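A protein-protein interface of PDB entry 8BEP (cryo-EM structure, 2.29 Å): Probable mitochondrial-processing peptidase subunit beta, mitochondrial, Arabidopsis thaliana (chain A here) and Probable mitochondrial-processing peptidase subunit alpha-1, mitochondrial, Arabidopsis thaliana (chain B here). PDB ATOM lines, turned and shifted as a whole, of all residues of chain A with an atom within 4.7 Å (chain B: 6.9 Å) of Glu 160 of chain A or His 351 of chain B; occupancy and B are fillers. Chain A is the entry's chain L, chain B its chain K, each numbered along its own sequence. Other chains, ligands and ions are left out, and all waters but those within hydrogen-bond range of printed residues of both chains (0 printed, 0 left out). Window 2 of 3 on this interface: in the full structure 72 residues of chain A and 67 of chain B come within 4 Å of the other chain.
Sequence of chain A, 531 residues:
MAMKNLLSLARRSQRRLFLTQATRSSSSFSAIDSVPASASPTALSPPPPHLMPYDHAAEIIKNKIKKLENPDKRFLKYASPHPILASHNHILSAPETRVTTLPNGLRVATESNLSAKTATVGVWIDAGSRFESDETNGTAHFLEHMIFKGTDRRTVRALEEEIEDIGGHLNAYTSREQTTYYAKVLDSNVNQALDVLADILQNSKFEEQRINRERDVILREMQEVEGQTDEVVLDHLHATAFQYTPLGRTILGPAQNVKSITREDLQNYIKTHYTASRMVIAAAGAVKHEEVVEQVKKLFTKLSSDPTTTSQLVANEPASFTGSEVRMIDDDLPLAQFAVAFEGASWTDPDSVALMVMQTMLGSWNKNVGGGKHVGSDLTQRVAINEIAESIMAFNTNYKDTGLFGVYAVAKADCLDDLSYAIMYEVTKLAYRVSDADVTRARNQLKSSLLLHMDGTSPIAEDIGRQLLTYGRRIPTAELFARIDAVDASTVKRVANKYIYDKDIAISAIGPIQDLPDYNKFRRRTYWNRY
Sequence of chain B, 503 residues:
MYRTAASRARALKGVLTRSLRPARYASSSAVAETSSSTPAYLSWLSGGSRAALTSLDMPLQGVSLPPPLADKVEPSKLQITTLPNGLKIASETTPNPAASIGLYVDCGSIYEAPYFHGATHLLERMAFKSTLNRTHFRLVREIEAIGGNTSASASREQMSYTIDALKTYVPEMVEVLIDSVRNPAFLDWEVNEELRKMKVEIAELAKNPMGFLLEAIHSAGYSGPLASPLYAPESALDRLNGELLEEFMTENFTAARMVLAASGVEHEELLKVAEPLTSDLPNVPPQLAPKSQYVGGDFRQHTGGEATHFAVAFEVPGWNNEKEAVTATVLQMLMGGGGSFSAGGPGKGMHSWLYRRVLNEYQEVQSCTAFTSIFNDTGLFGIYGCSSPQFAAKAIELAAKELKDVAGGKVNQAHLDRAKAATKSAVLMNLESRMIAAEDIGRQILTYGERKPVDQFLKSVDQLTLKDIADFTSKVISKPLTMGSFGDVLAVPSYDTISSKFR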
ATOM      1  N   VAL A 156      33.458  16.196  -8.121  1.00  0.00           N
ATOM      2  CA  VAL A 156      33.059  16.682  -9.462  1.00  0.00           C
ATOM      3  C   VAL A 156      31.536  16.638  -9.583  1.00  0.00           C
ATOM      4  O   VAL A 156      30.968  17.687  -9.921  1.00  0.00           O
ATOM      5  CB  VAL A 156      33.712  15.872 -10.596  1.00  0.00           C
ATOM      6  CG1 VAL A 156      35.218  16.026 -10.592  1.00  0.00           C
ATOM      7  CG2 VAL A 156      33.323  14.409 -10.544  1.00  0.00           C
ATOM      8  N   ARG A 157      30.936  15.476  -9.375  1.00  0.00           N
ATOM      9  CA  ARG A 157      29.494  15.449  -9.565  1.00  0.00           C
ATOM     10  C   ARG A 157      28.811  16.402  -8.601  1.00  0.00           C
ATOM     11  O   ARG A 157      28.158  17.346  -9.042  1.00  0.00           O
ATOM     12  CB  ARG A 157      28.955  14.025  -9.427  1.00  0.00           C
ATOM     13  CG  ARG A 157      28.858  13.303 -10.765  1.00  0.00           C
ATOM     14  CD  ARG A 157      28.764  11.791 -10.625  1.00  0.00           C
ATOM     15  NE  ARG A 157      29.581  11.265  -9.537  1.00  0.00           N
ATOM     16  CZ  ARG A 157      29.521  10.015  -9.098  1.00  0.00           C
ATOM     17  NH1 ARG A 157      28.686   9.136  -9.628  1.00  0.00           N
ATOM     18  NH2 ARG A 157      30.318   9.637  -8.104  1.00  0.00           N
ATOM     19  N   ALA A 158      29.052  16.210  -7.329  1.00  0.00           N
ATOM     20  CA  ALA A 158      28.495  17.086  -6.302  1.00  0.00           C
ATOM     21  C   ALA A 158      28.516  18.571  -6.714  1.00  0.00           C
ATOM     22  O   ALA A 158      27.490  19.214  -6.528  1.00  0.00           O
ATOM     23  CB  ALA A 158      29.360  16.840  -5.118  1.00  0.00           C
ATOM     24  N   LEU A 159      29.659  19.079  -7.205  1.00  0.00           N
ATOM     25  CA  LEU A 159      29.856  20.478  -7.659  1.00  0.00           C
ATOM     26  C   LEU A 159      29.070  20.773  -8.934  1.00  0.00           C
ATOM     27  O   LEU A 159      28.675  21.888  -9.072  1.00  0.00           O
ATOM     28  CB  LEU A 159      31.335  20.637  -7.991  1.00  0.00           C
ATOM     29  CG  LEU A 159      31.827  22.062  -8.215  1.00  0.00           C
ATOM     30  CD1 LEU A 159      32.365  22.636  -6.923  1.00  0.00           C
ATOM     31  CD2 LEU A 159      32.900  22.094  -9.283  1.00  0.00           C
ATOM     32  N   GLU A 160      28.935  19.819  -9.845  1.00  0.00           N
ATOM     33  CA  GLU A 160      28.116  20.039 -11.034  1.00  0.00           C
ATOM     34  C   GLU A 160      26.619  20.044 -10.738  1.00  0.00           C
ATOM     35  O   GLU A 160      25.910  20.940 -11.208  1.00  0.00           O
ATOM     36  CB  GLU A 160      28.425  18.975 -12.085  1.00  0.00           C
ATOM     37  CG  GLU A 160      29.738  19.188 -12.806  1.00  0.00           C
ATOM     38  CD  GLU A 160      29.822  18.405 -14.097  1.00  0.00           C
ATOM     39  OE1 GLU A 160      29.435  17.218 -14.097  1.00  0.00           O
ATOM     40  OE2 GLU A 160      30.272  18.976 -15.111  1.00  0.00           O
ATOM     41  N   GLU A 161      26.136  19.074  -9.965  1.00  0.00           N
ATOM     42  CA  GLU A 161      24.741  19.023  -9.548  1.00  0.00           C
ATOM     43  C   GLU A 161      24.345  20.239  -8.727  1.00  0.00           C
ATOM     44  O   GLU A 161      23.247  20.752  -8.912  1.00  0.00           O
ATOM     45  CB  GLU A 161      24.436  17.745  -8.756  1.00  0.00           C
ATOM     46  CG  GLU A 161      25.378  16.591  -9.009  1.00  0.00           C
ATOM     47  CD  GLU A 161      24.868  15.267  -8.472  1.00  0.00           C
ATOM     48  OE1 GLU A 161      25.656  14.299  -8.448  1.00  0.00           O
ATOM     49  OE2 GLU A 161      23.686  15.194  -8.076  1.00  0.00           O
ATOM     50  N   GLU A 162      25.168  20.762  -7.835  1.00  0.00           N
ATOM     51  CA  GLU A 162      24.719  21.960  -7.086  1.00  0.00           C
ATOM     52  C   GLU A 162      24.758  23.225  -7.966  1.00  0.00           C
ATOM     53  O   GLU A 162      23.956  24.112  -7.795  1.00  0.00           O
ATOM     54  CB  GLU A 162      25.520  22.135  -5.793  1.00  0.00           C
ATOM     55  CG  GLU A 162      25.711  23.542  -5.288  1.00  0.00           C
ATOM     56  CD  GLU A 162      27.000  23.697  -4.504  1.00  0.00           C
ATOM     57  OE1 GLU A 162      27.961  22.978  -4.821  1.00  0.00           O
ATOM     58  OE2 GLU A 162      27.036  24.528  -3.569  1.00  0.00           O
ATOM     59  N   ILE A 163      25.683  23.335  -8.888  1.00  0.00           N
ATOM     60  CA  ILE A 163      25.607  24.470  -9.804  1.00  0.00           C
ATOM     61  C   ILE A 163      24.350  24.378 -10.659  1.00  0.00           C
ATOM     62  O   ILE A 163      23.675  25.385 -10.907  1.00  0.00           O
ATOM     63  CB  ILE A 163      26.882  24.556 -10.663  1.00  0.00           C
ATOM     64  CG1 ILE A 163      28.096  24.876  -9.788  1.00  0.00           C
ATOM     65  CG2 ILE A 163      26.728  25.608 -11.751  1.00  0.00           C
ATOM     66  CD1 ILE A 163      27.850  25.957  -8.758  1.00  0.00           C
ATOM     67  N   GLU A 164      23.996  23.169 -11.100  1.00  0.00           N
ATOM     68  CA  GLU A 164      22.797  23.019 -11.919  1.00  0.00           C
ATOM     69  C   GLU A 164      21.523  23.189 -11.100  1.00  0.00           C
ATOM     70  O   GLU A 164      20.509  23.673 -11.617  1.00  0.00           O
ATOM     71  CB  GLU A 164      22.807  21.663 -12.614  1.00  0.00           C
ATOM     72  CG  GLU A 164      23.884  21.535 -13.654  1.00  0.00           C
ATOM     73  CD  GLU A 164      23.984  20.135 -14.192  1.00  0.00           C
ATOM     74  OE1 GLU A 164      23.867  19.187 -13.389  1.00  0.00           O
ATOM     75  OE2 GLU A 164      24.179  19.983 -15.415  1.00  0.00           O
ATOM     76  N   LEU B 334      15.605  19.996 -20.812  1.00  0.00           N
ATOM     77  CA  LEU B 334      15.744  18.661 -20.239  1.00  0.00           C
ATOM     78  C   LEU B 334      16.826  17.871 -20.962  1.00  0.00           C
ATOM     79  O   LEU B 334      17.668  17.223 -20.330  1.00  0.00           O
ATOM     80  CB  LEU B 334      14.403  17.931 -20.305  1.00  0.00           C
ATOM     81  CG  LEU B 334      13.988  16.938 -19.220  1.00  0.00           C
ATOM     82  CD1 LEU B 334      14.566  17.301 -17.861  1.00  0.00           C
ATOM     83  CD2 LEU B 334      12.473  16.863 -19.153  1.00  0.00           C
ATOM     84  N   MET B 335      16.819  17.911 -22.294  1.00  0.00           N
ATOM     85  CA  MET B 335      17.912  17.327 -23.057  1.00  0.00           C
ATOM     86  C   MET B 335      19.128  18.238 -23.126  1.00  0.00           C
ATOM     87  O   MET B 335      20.257  17.737 -23.137  1.00  0.00           O
ATOM     88  CB  MET B 335      17.450  16.987 -24.470  1.00  0.00           C
ATOM     89  CG  MET B 335      16.656  15.710 -24.552  1.00  0.00           C
ATOM     90  SD  MET B 335      14.880  15.960 -24.607  1.00  0.00           S
ATOM     91  CE  MET B 335      14.376  14.292 -24.981  1.00  0.00           C
ATOM     92  N   GLY B 345      35.015  24.824 -19.116  1.00  0.00           N
ATOM     93  CA  GLY B 345      34.931  24.291 -17.778  1.00  0.00           C
ATOM     94  C   GLY B 345      33.517  23.885 -17.421  1.00  0.00           C
ATOM     95  O   GLY B 345      32.543  24.356 -18.016  1.00  0.00           O
ATOM     96  N   PRO B 346      33.378  22.988 -16.447  1.00  0.00           N
ATOM     97  CA  PRO B 346      32.041  22.573 -16.006  1.00  0.00           C
ATOM     98  C   PRO B 346      31.273  23.733 -15.391  1.00  0.00           C
ATOM     99  O   PRO B 346      31.770  24.850 -15.244  1.00  0.00           O
ATOM    100  CB  PRO B 346      32.327  21.476 -14.975  1.00  0.00           C
ATOM    101  CG  PRO B 346      33.708  20.998 -15.299  1.00  0.00           C
ATOM    102  CD  PRO B 346      34.442  22.205 -15.799  1.00  0.00           C
ATOM    103  N   GLY B 347      30.025  23.449 -15.028  1.00  0.00           N
ATOM    104  CA  GLY B 347      29.129  24.457 -14.507  1.00  0.00           C
ATOM    105  C   GLY B 347      28.219  25.086 -15.540  1.00  0.00           C
ATOM    106  O   GLY B 347      27.321  25.849 -15.164  1.00  0.00           O
ATOM    107  N   LYS B 348      28.422  24.792 -16.823  1.00  0.00           N
ATOM    108  CA  LYS B 348      27.520  25.252 -17.871  1.00  0.00           C
ATOM    109  C   LYS B 348      26.322  24.331 -18.067  1.00  0.00           C
ATOM    110  O   LYS B 348      25.461  24.632 -18.901  1.00  0.00           O
ATOM    111  CB  LYS B 348      28.275  25.397 -19.195  1.00  0.00           C
ATOM    112  CG  LYS B 348      29.769  25.621 -19.048  1.00  0.00           C
ATOM    113  CD  LYS B 348      30.240  26.768 -19.927  1.00  0.00           C
ATOM    114  CE  LYS B 348      31.713  27.070 -19.705  1.00  0.00           C
ATOM    115  NZ  LYS B 348      32.220  28.075 -20.678  1.00  0.00           N
ATOM    116  N   GLY B 349      26.246  23.225 -17.331  1.00  0.00           N
ATOM    117  CA  GLY B 349      25.113  22.326 -17.430  1.00  0.00           C
ATOM    118  C   GLY B 349      25.354  21.119 -18.313  1.00  0.00           C
ATOM    119  O   GLY B 349      24.514  20.785 -19.155  1.00  0.00           O
ATOM    120  N   MET B 350      26.497  20.454 -18.131  1.00  0.00           N
ATOM    121  CA  MET B 350      26.822  19.290 -18.947  1.00  0.00           C
ATOM    122  C   MET B 350      25.977  18.068 -18.606  1.00  0.00           C
ATOM    123  O   MET B 350      25.929  17.131 -19.410  1.00  0.00           O
ATOM    124  CB  MET B 350      28.309  18.951 -18.816  1.00  0.00           C
ATOM    125  CG  MET B 350      28.624  17.821 -17.847  1.00  0.00           C
ATOM    126  SD  MET B 350      30.376  17.392 -17.839  1.00  0.00           S
ATOM    127  CE  MET B 350      30.556  16.663 -19.465  1.00  0.00           C
ATOM    128  N   HIS B 351      25.308  18.052 -17.451  1.00  0.00           N
ATOM    129  CA  HIS B 351      24.439  16.933 -17.106  1.00  0.00           C
ATOM    130  C   HIS B 351      23.120  16.955 -17.866  1.00  0.00           C
ATOM    131  O   HIS B 351      22.320  16.027 -17.702  1.00  0.00           O
ATOM    132  CB  HIS B 351      24.162  16.907 -15.602  1.00  0.00           C
ATOM    133  CG  HIS B 351      25.235  16.240 -14.800  1.00  0.00           C
ATOM    134  ND1 HIS B 351      24.973  15.219 -13.912  1.00  0.00           N
ATOM    135  CD2 HIS B 351      26.572  16.444 -14.753  1.00  0.00           C
ATOM    136  CE1 HIS B 351      26.102  14.825 -13.351  1.00  0.00           C
ATOM    137  NE2 HIS B 351      27.088  15.553 -13.845  1.00  0.00           N
ATOM    138  N   SER B 352      22.866  17.990 -18.668  1.00  0.00           N
ATOM    139  CA  SER B 352      21.715  17.987 -19.559  1.00  0.00           C
ATOM    140  C   SER B 352      21.763  16.752 -20.448  1.00  0.00           C
ATOM    141  O   SER B 352      22.831  16.355 -20.921  1.00  0.00           O
ATOM    142  CB  SER B 352      21.702  19.258 -20.411  1.00  0.00           C
ATOM    143  OG  SER B 352      21.255  20.374 -19.663  1.00  0.00           O
ATOM    144  N   TRP B 353      20.601  16.143 -20.682  1.00  0.00           N
ATOM    145  CA  TRP B 353      20.613  14.785 -21.210  1.00  0.00           C
ATOM    146  C   TRP B 353      20.848  14.751 -22.714  1.00  0.00           C
ATOM    147  O   TRP B 353      20.156  14.031 -23.442  1.00  0.00           O
ATOM    148  CB  TRP B 353      19.294  14.081 -20.886  1.00  0.00           C
ATOM    149  CG  TRP B 353      19.224  13.515 -19.503  1.00  0.00           C
ATOM    150  CD1 TRP B 353      18.364  13.883 -18.512  1.00  0.00           C
ATOM    151  CD2 TRP B 353      20.053  12.485 -18.954  1.00  0.00           C
ATOM    152  NE1 TRP B 353      18.599  13.139 -17.382  1.00  0.00           N
ATOM    153  CE2 TRP B 353      19.634  12.276 -17.625  1.00  0.00           C
ATOM    154  CE3 TRP B 353      21.108  11.718 -19.454  1.00  0.00           C
ATOM    155  CZ2 TRP B 353      20.232  11.331 -16.794  1.00  0.00           C
ATOM    156  CZ3 TRP B 353      21.701  10.781 -18.627  1.00  0.00           C
ATOM    157  CH2 TRP B 353      21.261  10.596 -17.312  1.00  0.00           C
ATOM    158  N   LEU B 354      21.813  15.520 -23.182  1.00  0.00           N
ATOM    159  CA  LEU B 354      22.525  15.291 -24.433  1.00  0.00           C
ATOM    160  C   LEU B 354      24.028  15.450 -24.269  1.00  0.00           C
ATOM    161  O   LEU B 354      24.792  14.696 -24.876  1.00  0.00           O
ATOM    162  CB  LEU B 354      22.011  16.229 -25.532  1.00  0.00           C
ATOM    163  CG  LEU B 354      20.751  15.754 -26.254  1.00  0.00           C
ATOM    164  CD1 LEU B 354      20.036  16.921 -26.914  1.00  0.00           C
ATOM    165  CD2 LEU B 354      21.092  14.680 -27.275  1.00  0.00           C
ATOM    166  N   TYR B 355      24.461  16.423 -23.465  1.00  0.00           N
ATOM    167  CA  TYR B 355      25.916  16.665 -23.274  1.00  0.00           C
ATOM    168  C   TYR B 355      26.535  15.460 -22.557  1.00  0.00           C
ATOM    169  O   TYR B 355      27.576  14.962 -23.024  1.00  0.00           O
ATOM    170  CB  TYR B 355      26.133  17.967 -22.497  1.00  0.00           C
ATOM    171  CG  TYR B 355      27.463  18.646 -22.710  1.00  0.00           C
ATOM    172  CD1 TYR B 355      28.658  17.981 -22.492  1.00  0.00           C
ATOM    173  CD2 TYR B 355      27.528  19.973 -23.104  1.00  0.00           C
ATOM    174  CE1 TYR B 355      29.881  18.605 -22.682  1.00  0.00           C
ATOM    175  CE2 TYR B 355      28.740  20.613 -23.298  1.00  0.00           C
ATOM    176  CZ  TYR B 355      29.922  19.928 -23.085  1.00  0.00           C
ATOM    177  OH  TYR B 355      31.122  20.552 -23.272  1.00  0.00           O
ATOM    178  N   ARG B 356      25.910  14.993 -21.473  1.00  0.00           N
ATOM    179  CA  ARG B 356      26.438  13.889 -20.686  1.00  0.00           C
ATOM    180  C   ARG B 356      26.135  12.535 -21.316  1.00  0.00           C
ATOM    181  O   ARG B 356      26.556  11.502 -20.782  1.00  0.00           O
ATOM    182  CB  ARG B 356      25.880  13.948 -19.258  1.00  0.00           C
ATOM    183  CG  ARG B 356      26.649  13.118 -18.238  1.00  0.00           C
ATOM    184  CD  ARG B 356      26.070  13.267 -16.842  1.00  0.00           C
ATOM    185  NE  ARG B 356      26.697  12.352 -15.896  1.00  0.00           N
ATOM    186  CZ  ARG B 356      26.294  11.108 -15.677  1.00  0.00           C
ATOM    187  NH1 ARG B 356      25.260  10.593 -16.322  1.00  0.00           N
ATOM    188  NH2 ARG B 356      26.945  10.362 -14.789  1.00  0.00           N
ATOM    189  N   ARG B 357      25.427  12.511 -22.444  1.00  0.00           N
ATOM    190  CA  ARG B 357      25.096  11.268 -23.122  1.00  0.00           C
ATOM    191  C   ARG B 357      25.871  11.105 -24.423  1.00  0.00           C
ATOM    192  O   ARG B 357      26.623  10.139 -24.574  1.00  0.00           O
ATOM    193  CB  ARG B 357      23.586  11.201 -23.390  1.00  0.00           C
ATOM    194  CG  ARG B 357      22.776  10.644 -22.235  1.00  0.00           C
ATOM    195  CD  ARG B 357      21.805   9.572 -22.699  1.00  0.00           C
ATOM    196  NE  ARG B 357      21.174   8.885 -21.578  1.00  0.00           N
ATOM    197  CZ  ARG B 357      19.922   9.082 -21.190  1.00  0.00           C
ATOM    198  NH1 ARG B 357      19.131   9.940 -21.812  1.00  0.00           N
ATOM    199  NH2 ARG B 357      19.450   8.401 -20.148  1.00  0.00           N
ATOM    200  N   HIS B 415      16.494  15.691 -12.268  1.00  0.00           N
ATOM    201  CA  HIS B 415      16.704  16.233 -13.604  1.00  0.00           C
ATOM    202  C   HIS B 415      15.647  17.269 -13.966  1.00  0.00           C
ATOM    203  O   HIS B 415      15.968  18.276 -14.607  1.00  0.00           O
ATOM    204  CB  HIS B 415      16.733  15.097 -14.624  1.00  0.00           C
ATOM    205  CG  HIS B 415      17.812  14.091 -14.369  1.00  0.00           C
ATOM    206  ND1 HIS B 415      17.562  12.858 -13.808  1.00  0.00           N
ATOM    207  CD2 HIS B 415      19.148  14.146 -14.576  1.00  0.00           C
ATOM    208  CE1 HIS B 415      18.696  12.189 -13.695  1.00  0.00           C
ATOM    209  NE2 HIS B 415      19.674  12.950 -14.153  1.00  0.00           N
ATOM    210  N   ARG B 418      16.526  20.451 -12.184  1.00  0.00           N
ATOM    211  CA  ARG B 418      17.668  21.075 -12.847  1.00  0.00           C
ATOM    212  C   ARG B 418      17.238  21.786 -14.127  1.00  0.00           C
ATOM    213  O   ARG B 418      17.660  22.917 -14.394  1.00  0.00           O
ATOM    214  CB  ARG B 418      18.749  20.029 -13.133  1.00  0.00           C
ATOM    215  CG  ARG B 418      19.525  19.606 -11.892  1.00  0.00           C
ATOM    216  CD  ARG B 418      20.498  18.470 -12.180  1.00  0.00           C
ATOM    217  NE  ARG B 418      20.587  17.531 -11.067  1.00  0.00           N
ATOM    218  CZ  ARG B 418      21.272  16.396 -11.097  1.00  0.00           C
ATOM    219  NH1 ARG B 418      21.940  16.019 -12.176  1.00  0.00           N
ATOM    220  NH2 ARG B 418      21.289  15.619 -10.018  1.00  0.00           N
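SD of Met 350 of chain B sits close to OE2 of Glu 160 of chain A (3.2 Å). The backbone NH (N) of His 351 of chain B is in hydrogen-bond range of the side-chain carboxylate (OE2) of Glu 164 of chain A, at 3.0 Å. NE2 of His 351 of chain B lies within hydrogen-bond range of OE1 of Glu 160 of chain A (2.9 Å). The side-chain carboxylate (OE2) of Glu 161 of chain A lies within salt-bridge range of the guanidinium group (NH2) of Arg 418 of chain B, at 3.1 Å. NH1 of Arg 418 of chain B is in salt-bridge range of OE1 of Glu 164 of chain A, at 3.9 Å.
The side-chain hydroxyl (OG) of Ser 352 of chain B lies within hydrogen-bond range of the backbone carbonyl oxygen (O) of Gly 349 of chain B (3.3 Å). The backbone NH of Arg 356 of chain B is in hydrogen-bond range of the backbone carbonyl oxygen of Met 350 of chain B (3.0 Å).
Among the printed residues, pairs that only touch across the chains: Glu 160 of chain A with Pro 346 of chain B (3.2 Å), Ile 163 of chain A with Gly 347 of chain B (3.5 Å), Glu 164 of chain A with Gly 349 of chain B (3.2 Å) and Glu 164 of chain A with Met 350 of chain B (3.6 Å).
Of the printed residues of chain B, Glu 160 of chain A touches Pro 346 (3.2 Å), Met 350 (3.2 Å) and His 351 (2.9 Å). Printed residues of chain A within 4 Å of Pro 346 of chain B: Glu 160 (3.2 Å). Of the printed residues of chain A, Gly 347 of chain B touches Ile 163. Printed residues of chain A within 4 Å of Gly 349 of chain B: Glu 164 (3.2 Å). Of chain A, only Glu 160 (2.9 Å) and Glu 164 (3.0 Å) come within 4 Å of His 351 of chain B. Of the printed residues of chain A, Arg 418 of chain B touches Glu 161 and Glu 164.
Of the 9 printed residues of chain A, 4 touch a printed residue of chain B. Printed residues of chain A that touch a printed residue of chain B: Glu 160, Glu 161, Ile 163 and Glu 164. Of the 17 printed residues of chain B, 6 touch a printed residue of chain A. Hydrophobic or aromatic side chains of chain B that line the printed part of chain A: Pro 346, Met 350 and His 351.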
